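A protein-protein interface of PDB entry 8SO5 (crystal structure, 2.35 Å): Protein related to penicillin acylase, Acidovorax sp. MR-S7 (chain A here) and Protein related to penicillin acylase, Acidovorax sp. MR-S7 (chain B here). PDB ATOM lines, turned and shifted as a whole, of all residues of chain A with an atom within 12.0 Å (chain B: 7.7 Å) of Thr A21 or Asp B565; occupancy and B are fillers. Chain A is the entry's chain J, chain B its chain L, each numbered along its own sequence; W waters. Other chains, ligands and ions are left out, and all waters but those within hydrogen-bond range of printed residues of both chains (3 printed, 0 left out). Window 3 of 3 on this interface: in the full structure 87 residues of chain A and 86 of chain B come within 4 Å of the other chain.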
ATOM      1  N   ILE A  17     -11.060  -3.951   5.356  1.00  0.00           N
ATOM      2  CA  ILE A  17     -10.212  -4.752   6.219  1.00  0.00           C
ATOM      3  C   ILE A  17      -8.798  -4.178   6.196  1.00  0.00           C
ATOM      4  O   ILE A  17      -8.092  -4.296   5.198  1.00  0.00           O
ATOM      5  CB  ILE A  17     -10.243  -6.228   5.779  1.00  0.00           C
ATOM      6  CG1 ILE A  17     -11.655  -6.810   5.874  1.00  0.00           C
ATOM      7  CG2 ILE A  17      -9.237  -7.050   6.568  1.00  0.00           C
ATOM      8  CD1 ILE A  17     -11.787  -8.204   5.308  1.00  0.00           C
ATOM      9  N   ARG A  18      -8.406  -3.546   7.307  1.00  0.00           N
ATOM     10  CA  ARG A  18      -7.050  -3.055   7.476  1.00  0.00           C
ATOM     11  C   ARG A  18      -6.267  -4.065   8.310  1.00  0.00           C
ATOM     12  O   ARG A  18      -6.755  -4.534   9.335  1.00  0.00           O
ATOM     13  CB  ARG A  18      -7.047  -1.682   8.158  1.00  0.00           C
ATOM     14  CG  ARG A  18      -7.814  -0.599   7.411  1.00  0.00           C
ATOM     15  CD  ARG A  18      -9.313  -0.675   7.633  1.00  0.00           C
ATOM     16  NE  ARG A  18      -9.701  -0.358   9.002  1.00  0.00           N
ATOM     17  CZ  ARG A  18      -9.688   0.862   9.532  1.00  0.00           C
ATOM     18  NH1 ARG A  18      -9.321   1.900   8.804  1.00  0.00           N
ATOM     19  NH2 ARG A  18     -10.053   1.040  10.789  1.00  0.00           N
ATOM     20  N   ARG A  19      -5.055  -4.402   7.858  1.00  0.00           N
ATOM     21  CA  ARG A  19      -4.178  -5.270   8.626  1.00  0.00           C
ATOM     22  C   ARG A  19      -2.894  -4.523   8.969  1.00  0.00           C
ATOM     23  O   ARG A  19      -2.358  -3.781   8.148  1.00  0.00           O
ATOM     24  CB  ARG A  19      -3.870  -6.566   7.869  1.00  0.00           C
ATOM     25  CG  ARG A  19      -5.053  -7.518   7.776  1.00  0.00           C
ATOM     26  CD  ARG A  19      -4.616  -8.958   7.598  1.00  0.00           C
ATOM     27  NE  ARG A  19      -5.749  -9.861   7.445  1.00  0.00           N
ATOM     28  CZ  ARG A  19      -6.029 -10.868   8.264  1.00  0.00           C
ATOM     29  NH1 ARG A  19      -7.053 -11.661   8.004  1.00  0.00           N
ATOM     30  NH2 ARG A  19      -5.280 -11.090   9.330  1.00  0.00           N
ATOM     31  N   THR A  20      -2.418  -4.738  10.198  1.00  0.00           N
ATOM     32  CA  THR A  20      -1.210  -4.098  10.687  1.00  0.00           C
ATOM     33  C   THR A  20      -0.213  -5.179  11.096  1.00  0.00           C
ATOM     34  O   THR A  20      -0.373  -6.346  10.741  1.00  0.00           O
ATOM     35  CB  THR A  20      -1.540  -3.125  11.827  1.00  0.00           C
ATOM     36  OG1 THR A  20      -2.177  -3.849  12.881  1.00  0.00           O
ATOM     37  CG2 THR A  20      -2.439  -1.993  11.381  1.00  0.00           C
ATOM     38  N   THR A  21       0.816  -4.775  11.846  1.00  0.00           N
ATOM     39  CA  THR A  21       1.875  -5.681  12.253  1.00  0.00           C
ATOM     40  C   THR A  21       1.261  -6.907  12.922  1.00  0.00           C
ATOM     41  O   THR A  21       0.279  -6.795  13.653  1.00  0.00           O
ATOM     42  CB  THR A  21       2.879  -4.963  13.164  1.00  0.00           C
ATOM     43  OG1 THR A  21       3.219  -3.723  12.540  1.00  0.00           O
ATOM     44  CG2 THR A  21       4.132  -5.772  13.424  1.00  0.00           C
ATOM     45  N   MET A  22       1.848  -8.077  12.646  1.00  0.00           N
ATOM     46  CA  MET A  22       1.397  -9.340  13.209  1.00  0.00           C
ATOM     47  C   MET A  22       0.078  -9.747  12.556  1.00  0.00           C
ATOM     48  O   MET A  22      -0.530 -10.742  12.942  1.00  0.00           O
ATOM     49  CB  MET A  22       1.203  -9.231  14.724  1.00  0.00           C
ATOM     50  CG  MET A  22       2.447  -8.764  15.459  1.00  0.00           C
ATOM     51  SD  MET A  22       3.923  -9.728  15.048  1.00  0.00           S
ATOM     52  CE  MET A  22       5.069  -9.105  16.277  1.00  0.00           C
ATOM     53  N   GLY A  23      -0.358  -8.962  11.564  1.00  0.00           N
ATOM     54  CA  GLY A  23      -1.537  -9.287  10.779  1.00  0.00           C
ATOM     55  C   GLY A  23      -2.838  -8.948  11.505  1.00  0.00           C
ATOM     56  O   GLY A  23      -3.910  -9.391  11.100  1.00  0.00           O
ATOM     57  N   VAL A  24      -2.733  -8.156  12.576  1.00  0.00           N
ATOM     58  CA  VAL A  24      -3.898  -7.764  13.350  1.00  0.00           C
ATOM     59  C   VAL A  24      -4.890  -7.076  12.418  1.00  0.00           C
ATOM     60  O   VAL A  24      -4.585  -6.043  11.828  1.00  0.00           O
ATOM     61  CB  VAL A  24      -3.518  -6.850  14.530  1.00  0.00           C
ATOM     62  CG1 VAL A  24      -4.749  -6.334  15.259  1.00  0.00           C
ATOM     63  CG2 VAL A  24      -2.569  -7.539  15.499  1.00  0.00           C
ATOM     64  N   PRO A  25      -6.108  -7.637  12.250  1.00  0.00           N
ATOM     65  CA  PRO A  25      -7.129  -7.024  11.404  1.00  0.00           C
ATOM     66  C   PRO A  25      -7.932  -5.943  12.121  1.00  0.00           C
ATOM     67  O   PRO A  25      -8.355  -6.125  13.260  1.00  0.00           O
ATOM     68  CB  PRO A  25      -8.025  -8.221  11.060  1.00  0.00           C
ATOM     69  CG  PRO A  25      -7.964  -9.082  12.303  1.00  0.00           C
ATOM     70  CD  PRO A  25      -6.556  -8.910  12.836  1.00  0.00           C
ATOM     71  N   HIS A  26      -8.127  -4.816  11.433  1.00  0.00           N
ATOM     72  CA  HIS A  26      -8.995  -3.757  11.918  1.00  0.00           C
ATOM     73  C   HIS A  26     -10.155  -3.611  10.937  1.00  0.00           C
ATOM     74  O   HIS A  26      -9.977  -3.113   9.829  1.00  0.00           O
ATOM     75  CB  HIS A  26      -8.206  -2.456  12.108  1.00  0.00           C
ATOM     76  CG  HIS A  26      -6.888  -2.633  12.790  1.00  0.00           C
ATOM     77  ND1 HIS A  26      -6.651  -2.244  14.091  1.00  0.00           N
ATOM     78  CD2 HIS A  26      -5.738  -3.163  12.350  1.00  0.00           C
ATOM     79  CE1 HIS A  26      -5.396  -2.526  14.413  1.00  0.00           C
ATOM     80  NE2 HIS A  26      -4.822  -3.083  13.369  1.00  0.00           N
ATOM     81  N   ASP A  46      -7.889 -16.921   8.396  1.00  0.00           N
ATOM     82  CA  ASP A  46      -6.710 -17.203   9.198  1.00  0.00           C
ATOM     83  C   ASP A  46      -6.810 -18.577   9.860  1.00  0.00           C
ATOM     84  O   ASP A  46      -5.785 -19.183  10.161  1.00  0.00           O
ATOM     85  CB  ASP A  46      -6.471 -16.106  10.239  1.00  0.00           C
ATOM     86  CG  ASP A  46      -5.964 -14.799   9.652  1.00  0.00           C
ATOM     87  OD1 ASP A  46      -5.101 -14.858   8.754  1.00  0.00           O
ATOM     88  OD2 ASP A  46      -6.413 -13.734  10.115  1.00  0.00           O
ATOM     89  N   GLN B  34      -7.425 -12.054  17.772  1.00  0.00           N
ATOM     90  CA  GLN B  34      -7.335 -10.630  18.052  1.00  0.00           C
ATOM     91  C   GLN B  34      -7.809  -9.836  16.837  1.00  0.00           C
ATOM     92  O   GLN B  34      -7.466 -10.166  15.705  1.00  0.00           O
ATOM     93  CB  GLN B  34      -5.900 -10.247  18.423  1.00  0.00           C
ATOM     94  CG  GLN B  34      -5.756  -8.801  18.879  1.00  0.00           C
ATOM     95  CD  GLN B  34      -4.336  -8.433  19.229  1.00  0.00           C
ATOM     96  OE1 GLN B  34      -3.416  -9.240  19.115  1.00  0.00           O
ATOM     97  NE2 GLN B  34      -4.145  -7.198  19.663  1.00  0.00           N
ATOM     98  N   LEU B 529      -1.977 -15.499  15.084  1.00  0.00           N
ATOM     99  CA  LEU B 529      -3.366 -15.375  14.667  1.00  0.00           C
ATOM    100  C   LEU B 529      -3.823 -16.578  13.841  1.00  0.00           C
ATOM    101  O   LEU B 529      -4.986 -16.965  13.925  1.00  0.00           O
ATOM    102  CB  LEU B 529      -3.519 -14.071  13.874  1.00  0.00           C
ATOM    103  CG  LEU B 529      -3.795 -12.821  14.709  1.00  0.00           C
ATOM    104  CD1 LEU B 529      -3.457 -11.559  13.931  1.00  0.00           C
ATOM    105  CD2 LEU B 529      -5.247 -12.784  15.162  1.00  0.00           C
ATOM    106  N   HIS B 537       1.355 -15.233   9.388  1.00  0.00           N
ATOM    107  CA  HIS B 537       0.861 -14.845  10.698  1.00  0.00           C
ATOM    108  C   HIS B 537       0.663 -16.090  11.558  1.00  0.00           C
ATOM    109  O   HIS B 537      -0.252 -16.145  12.378  1.00  0.00           O
ATOM    110  CB  HIS B 537      -0.414 -14.006  10.559  1.00  0.00           C
ATOM    111  CG  HIS B 537      -0.227 -12.796   9.705  1.00  0.00           C
ATOM    112  ND1 HIS B 537       0.798 -11.898   9.912  1.00  0.00           N
ATOM    113  CD2 HIS B 537      -0.905 -12.347   8.641  1.00  0.00           C
ATOM    114  CE1 HIS B 537       0.724 -10.936   9.003  1.00  0.00           C
ATOM    115  NE2 HIS B 537      -0.304 -11.189   8.223  1.00  0.00           N
ATOM    116  N   ASP B 540       4.706 -15.033  13.678  1.00  0.00           N
ATOM    117  CA  ASP B 540       5.271 -13.696  13.779  1.00  0.00           C
ATOM    118  C   ASP B 540       5.064 -13.154  15.192  1.00  0.00           C
ATOM    119  O   ASP B 540       5.968 -12.549  15.766  1.00  0.00           O
ATOM    120  CB  ASP B 540       4.705 -12.762  12.705  1.00  0.00           C
ATOM    121  CG  ASP B 540       3.188 -12.711  12.639  1.00  0.00           C
ATOM    122  OD1 ASP B 540       2.539 -13.375  13.473  1.00  0.00           O
ATOM    123  OD2 ASP B 540       2.669 -12.011  11.748  1.00  0.00           O
ATOM    124  N   TYR B 541       3.872 -13.380  15.750  1.00  0.00           N
ATOM    125  CA  TYR B 541       3.552 -12.913  17.087  1.00  0.00           C
ATOM    126  C   TYR B 541       4.362 -13.724  18.097  1.00  0.00           C
ATOM    127  O   TYR B 541       4.870 -13.185  19.079  1.00  0.00           O
ATOM    128  CB  TYR B 541       2.050 -13.057  17.353  1.00  0.00           C
ATOM    129  CG  TYR B 541       1.375 -11.848  17.950  1.00  0.00           C
ATOM    130  CD1 TYR B 541       1.965 -11.110  18.962  1.00  0.00           C
ATOM    131  CD2 TYR B 541       0.123 -11.450  17.508  1.00  0.00           C
ATOM    132  CE1 TYR B 541       1.337 -10.002  19.510  1.00  0.00           C
ATOM    133  CE2 TYR B 541      -0.520 -10.349  18.047  1.00  0.00           C
ATOM    134  CZ  TYR B 541       0.089  -9.622  19.053  1.00  0.00           C
ATOM    135  OH  TYR B 541      -0.549  -8.529  19.587  1.00  0.00           O
ATOM    136  N   LEU B 551       3.620  -5.694  21.642  1.00  0.00           N
ATOM    137  CA  LEU B 551       3.203  -4.941  20.473  1.00  0.00           C
ATOM    138  C   LEU B 551       2.309  -3.785  20.909  1.00  0.00           C
ATOM    139  O   LEU B 551       1.281  -3.999  21.545  1.00  0.00           O
ATOM    140  CB  LEU B 551       2.450  -5.872  19.517  1.00  0.00           C
ATOM    141  CG  LEU B 551       1.900  -5.208  18.254  1.00  0.00           C
ATOM    142  CD1 LEU B 551       2.978  -5.096  17.186  1.00  0.00           C
ATOM    143  CD2 LEU B 551       0.693  -5.962  17.721  1.00  0.00           C
ATOM    144  N   ARG B 552       2.719  -2.560  20.565  1.00  0.00           N
ATOM    145  CA  ARG B 552       1.841  -1.409  20.677  1.00  0.00           C
ATOM    146  C   ARG B 552       0.847  -1.466  19.520  1.00  0.00           C
ATOM    147  O   ARG B 552       1.174  -1.094  18.395  1.00  0.00           O
ATOM    148  CB  ARG B 552       2.645  -0.105  20.673  1.00  0.00           C
ATOM    149  CG  ARG B 552       1.791   1.156  20.668  1.00  0.00           C
ATOM    150  CD  ARG B 552       0.839   1.231  21.849  1.00  0.00           C
ATOM    151  NE  ARG B 552      -0.100   2.339  21.733  1.00  0.00           N
ATOM    152  CZ  ARG B 552       0.241   3.624  21.751  1.00  0.00           C
ATOM    153  NH1 ARG B 552      -0.674   4.552  21.532  1.00  0.00           N
ATOM    154  NH2 ARG B 552       1.498   3.978  21.965  1.00  0.00           N
ATOM    155  N   VAL B 553      -0.360  -1.961  19.809  1.00  0.00           N
ATOM    156  CA  VAL B 553      -1.350  -2.217  18.777  1.00  0.00           C
ATOM    157  C   VAL B 553      -2.015  -0.901  18.387  1.00  0.00           C
ATOM    158  O   VAL B 553      -2.434  -0.131  19.249  1.00  0.00           O
ATOM    159  CB  VAL B 553      -2.391  -3.255  19.241  1.00  0.00           C
ATOM    160  CG1 VAL B 553      -3.198  -2.755  20.429  1.00  0.00           C
ATOM    161  CG2 VAL B 553      -3.311  -3.670  18.104  1.00  0.00           C
ATOM    162  N   PRO B 554      -2.127  -0.608  17.072  1.00  0.00           N
ATOM    163  CA  PRO B 554      -2.787   0.610  16.600  1.00  0.00           C
ATOM    164  C   PRO B 554      -4.281   0.588  16.916  1.00  0.00           C
ATOM    165  O   PRO B 554      -4.910  -0.468  16.872  1.00  0.00           O
ATOM    166  CB  PRO B 554      -2.555   0.603  15.080  1.00  0.00           C
ATOM    167  CG  PRO B 554      -1.445  -0.410  14.857  1.00  0.00           C
ATOM    168  CD  PRO B 554      -1.611  -1.426  15.967  1.00  0.00           C
ATOM    169  N   ILE B 560      -3.562   3.406  12.677  1.00  0.00           N
ATOM    170  CA  ILE B 560      -3.764   2.265  11.800  1.00  0.00           C
ATOM    171  C   ILE B 560      -3.164   2.560  10.427  1.00  0.00           C
ATOM    172  O   ILE B 560      -2.470   1.719   9.861  1.00  0.00           O
ATOM    173  CB  ILE B 560      -5.262   1.915  11.703  1.00  0.00           C
ATOM    174  CG1 ILE B 560      -5.801   1.388  13.036  1.00  0.00           C
ATOM    175  CG2 ILE B 560      -5.513   0.936  10.567  1.00  0.00           C
ATOM    176  CD1 ILE B 560      -7.290   1.130  13.039  1.00  0.00           C
ATOM    177  N   THR B 561      -3.443   3.755   9.898  1.00  0.00           N
ATOM    178  CA  THR B 561      -2.983   4.134   8.573  1.00  0.00           C
ATOM    179  C   THR B 561      -1.478   4.390   8.603  1.00  0.00           C
ATOM    180  O   THR B 561      -0.796   4.214   7.596  1.00  0.00           O
ATOM    181  CB  THR B 561      -3.759   5.349   8.047  1.00  0.00           C
ATOM    182  OG1 THR B 561      -3.664   6.403   9.005  1.00  0.00           O
ATOM    183  CG2 THR B 561      -5.217   5.046   7.782  1.00  0.00           C
ATOM    184  N   GLY B 562      -0.969   4.795   9.771  1.00  0.00           N
ATOM    185  CA  GLY B 562       0.434   5.144   9.923  1.00  0.00           C
ATOM    186  C   GLY B 562       1.306   3.928  10.228  1.00  0.00           C
ATOM    187  O   GLY B 562       2.531   4.021  10.213  1.00  0.00           O
ATOM    188  N   ASN B 563       0.662   2.789  10.503  1.00  0.00           N
ATOM    189  CA  ASN B 563       1.372   1.560  10.823  1.00  0.00           C
ATOM    190  C   ASN B 563       2.275   1.181   9.654  1.00  0.00           C
ATOM    191  O   ASN B 563       1.928   1.404   8.497  1.00  0.00           O
ATOM    192  CB  ASN B 563       0.410   0.417  11.155  1.00  0.00           C
ATOM    193  CG  ASN B 563       1.123  -0.881  11.466  1.00  0.00           C
ATOM    194  OD1 ASN B 563       1.120  -1.807  10.657  1.00  0.00           O
ATOM    195  ND2 ASN B 563       1.748  -0.954  12.630  1.00  0.00           N
ATOM    196  N   ALA B 564       3.428   0.587   9.976  1.00  0.00           N
ATOM    197  CA  ALA B 564       4.462   0.306   8.993  1.00  0.00           C
ATOM    198  C   ALA B 564       4.026  -0.811   8.047  1.00  0.00           C
ATOM    199  O   ALA B 564       4.552  -0.926   6.943  1.00  0.00           O
ATOM    200  CB  ALA B 564       5.747  -0.051   9.700  1.00  0.00           C
ATOM    201  N   ASP B 565       3.065  -1.632   8.486  1.00  0.00           N
ATOM    202  CA  ASP B 565       2.654  -2.800   7.723  1.00  0.00           C
ATOM    203  C   ASP B 565       1.217  -2.625   7.237  1.00  0.00           C
ATOM    204  O   ASP B 565       0.531  -3.606   6.957  1.00  0.00           O
ATOM    205  CB  ASP B 565       2.804  -4.076   8.557  1.00  0.00           C
ATOM    206  CG  ASP B 565       4.214  -4.310   9.069  1.00  0.00           C
ATOM    207  OD1 ASP B 565       5.123  -4.470   8.229  1.00  0.00           O
ATOM    208  OD2 ASP B 565       4.394  -4.326  10.305  1.00  0.00           O
ATOM    209  N   TYR B 566       0.785  -1.365   7.118  1.00  0.00           N
ATOM    210  CA  TYR B 566      -0.594  -1.036   6.796  1.00  0.00           C
ATOM    211  C   TYR B 566      -0.950  -1.513   5.389  1.00  0.00           C
ATOM    212  O   TYR B 566      -0.282  -1.160   4.421  1.00  0.00           O
ATOM    213  CB  TYR B 566      -0.816   0.473   6.929  1.00  0.00           C
ATOM    214  CG  TYR B 566      -2.152   0.969   6.433  1.00  0.00           C
ATOM    215  CD1 TYR B 566      -3.337   0.505   6.979  1.00  0.00           C
ATOM    216  CD2 TYR B 566      -2.233   1.909   5.419  1.00  0.00           C
ATOM    217  CE1 TYR B 566      -4.568   0.957   6.529  1.00  0.00           C
ATOM    218  CE2 TYR B 566      -3.454   2.374   4.959  1.00  0.00           C
ATOM    219  CZ  TYR B 566      -4.627   1.897   5.515  1.00  0.00           C
ATOM    220  OH  TYR B 566      -5.839   2.358   5.059  1.00  0.00           O
ATOM    221  N   ARG B 567      -2.016  -2.318   5.300  1.00  0.00           N
ATOM    222  CA  ARG B 567      -2.632  -2.663   4.029  1.00  0.00           C
ATOM    223  C   ARG B 567      -4.147  -2.707   4.218  1.00  0.00           C
ATOM    224  O   ARG B 567      -4.635  -3.185   5.240  1.00  0.00           O
ATOM    225  CB  ARG B 567      -2.105  -4.001   3.497  1.00  0.00           C
ATOM    226  CG  ARG B 567      -0.607  -4.201   3.678  1.00  0.00           C
ATOM    227  CD  ARG B 567       0.068  -4.839   2.478  1.00  0.00           C
ATOM    228  NE  ARG B 567       0.423  -3.844   1.476  1.00  0.00           N
ATOM    229  CZ  ARG B 567       1.652  -3.376   1.284  1.00  0.00           C
ATOM    230  NH1 ARG B 567       2.645  -3.790   2.051  1.00  0.00           N
ATOM    231  NH2 ARG B 567       1.883  -2.483   0.337  1.00  0.00           N
ATOM    232  N   THR B 568      -4.885  -2.193   3.227  1.00  0.00           N
ATOM    233  CA  THR B 568      -6.336  -2.160   3.300  1.00  0.00           C
ATOM    234  C   THR B 568      -6.929  -2.860   2.083  1.00  0.00           C
ATOM    235  O   THR B 568      -6.342  -2.857   1.003  1.00  0.00           O
ATOM    236  CB  THR B 568      -6.867  -0.724   3.415  1.00  0.00           C
ATOM    237  OG1 THR B 568      -8.259  -0.790   3.730  1.00  0.00           O
ATOM    238  CG2 THR B 568      -6.674   0.087   2.153  1.00  0.00           C
HETATM  239  O   HOH W   1       0.177 -13.130  14.216  1.00  0.00           O
HETATM  240  O   HOH W   2      -8.464   2.634   6.526  1.00  0.00           O
HETATM  241  O   HOH W   3      -0.063  -6.504   7.633  1.00  0.00           O
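Water W1 lies within hydrogen-bond range of the side-chain carboxylate of Asp B540 (2.5 Å), the backbone carbonyl oxygen of Met A22 (2.8 Å) and the backbone NH of Leu B529 (3.3 Å).
Water W2 lies within hydrogen-bond range of NH1 of Arg A18 (2.5 Å) and OH of Tyr B566 (3.0 Å).
Water W3 bridges the backbone carbonyl oxygen (O) of Asp B565 and the backbone carbonyl oxygen (O) of Thr A20.
Printed residues of chain B within 4 Å of Thr A21: Leu B551, Asn B563 and Asp B565.
Asp B565 touches two residues of chain A.
No residue of chain A comes within 4 Å of Gly B562.
Of chain A, only Thr A20 and Thr A21 come within 4 Å of Asn B563.
No residue of chain A comes within 4 Å of Ala B564.
Arg B567 touches three residues of chain A.
Printed residues of chain B within 4 Å of Ile A17: Arg B567 and Thr B568.
Of the printed residues of chain B, Gly A23 touches Leu B529 (3.6 Å) and His B537 (3.3 Å).
Printed residues of chain B within 4 Å of Thr A20: Pro B554 and Asn B563.
Of the printed residues of chain A, Leu B551 touches Thr A21 (3.99 Å).
Thr B561 touches none of the printed residues of chain A.
The nearest printed residue of chain B that does not touch Thr A21 is Ala B564 (5.0 Å).
The nearest printed residue of chain B that does not touch Gly A23 is Asp B540 (4.3 Å).
The backbone NH (N) of Arg A19 is in hydrogen-bond range of the backbone carbonyl oxygen (O) of Arg B567.
The backbone carbonyl oxygen (O) of Arg A19 lies close to the backbone carbonyl oxygen (O) of Asp B565 (3.1 Å).
OG1 of Thr A21 is in hydrogen-bond range of ND2 of Asn B563, 3.1 Å away.
SD of Met A22 lies within hydrogen-bond range of N of Tyr B541, 3.7 Å away.
OG1 of Thr A21 sits at hydrogen-bond distance from OD2 of Asp B565 (2.6 Å).
SD of Met A22 sits close to O of Asp B540, 3.6 Å away.
Among the printed residues, pairs that only touch across the chains: Ile A17 with Arg B567 (3.6 Å), Ile A17 with Thr B568 (3.4 Å), Arg A18 with Ile B560 (3.6 Å), Arg A18 with Tyr B566 (3.7 Å), Arg A18 with Arg B567 (3.3 Å), Arg A18 with Thr B568 (3.7 Å), Arg A19 with Tyr B566 (3.5 Å), Thr A20 with Pro B554 (3.9 Å), Thr A20 with Asn B563 (3.2 Å), Thr A21 with Leu B551 (3.99 Å), Met A22 with Leu B529 (3.2 Å), Met A22 with His B537 (3.5 Å), Gly A23 with Leu B529 (3.6 Å), Gly A23 with His B537 (3.3 Å), Val A24 with Leu B529 (3.7 Å), Pro A25 with Gln B34 (3.3 Å), His A26 with Pro B554 (3.2 Å) and His A26 with Ile B560 (3.6 Å).
Of the 11 printed residues of chain A, 10 touch a printed residue of chain B.
Hydrophobic or aromatic side chains of chain A that line the printed part of chain B: Met A22, Pro A25 and His A26.
Hydrophobic or aromatic side chains of chain B within 4 Å of the printed part of chain A: Leu B529, His B537, Tyr B541, Leu B551, Pro B554, Ile B560 and Tyr B566.
Along chain B the printed residues that touch a printed residue of chain A span positions 34 to 568.
Among the printed residues, no Asp or Glu carboxylate lies within 4 Å of a Lys or Arg side-chain nitrogen of the other chain.
The backbone carbonyl oxygen (O) of Val A24 sits at hydrogen-bond distance from the side-chain hydroxyl (OG1) of Thr A20, at 3.4 Å.
The side-chain hydroxyl (OH) of Tyr B541 is in hydrogen-bond range of the side-chain amide oxygen (OE1) of Gln B34 (3.0 Å).
The guanidinium group of Arg A19 sits at hydrogen-bond distance from the backbone carbonyl oxygen of Gly A23 (2.8 Å).
The side-chain amide oxygen (OD1) of Asn B563 is in hydrogen-bond range of the backbone NH (N) of Asp B565 (2.9 Å).
N of Leu B529 is in hydrogen-bond range of O of His B537, at 3.3 Å.
The side-chain hydroxyl (OG1) of Thr A20 lies within hydrogen-bond range of a ring nitrogen (NE2) of His A26, 2.8 Å away.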
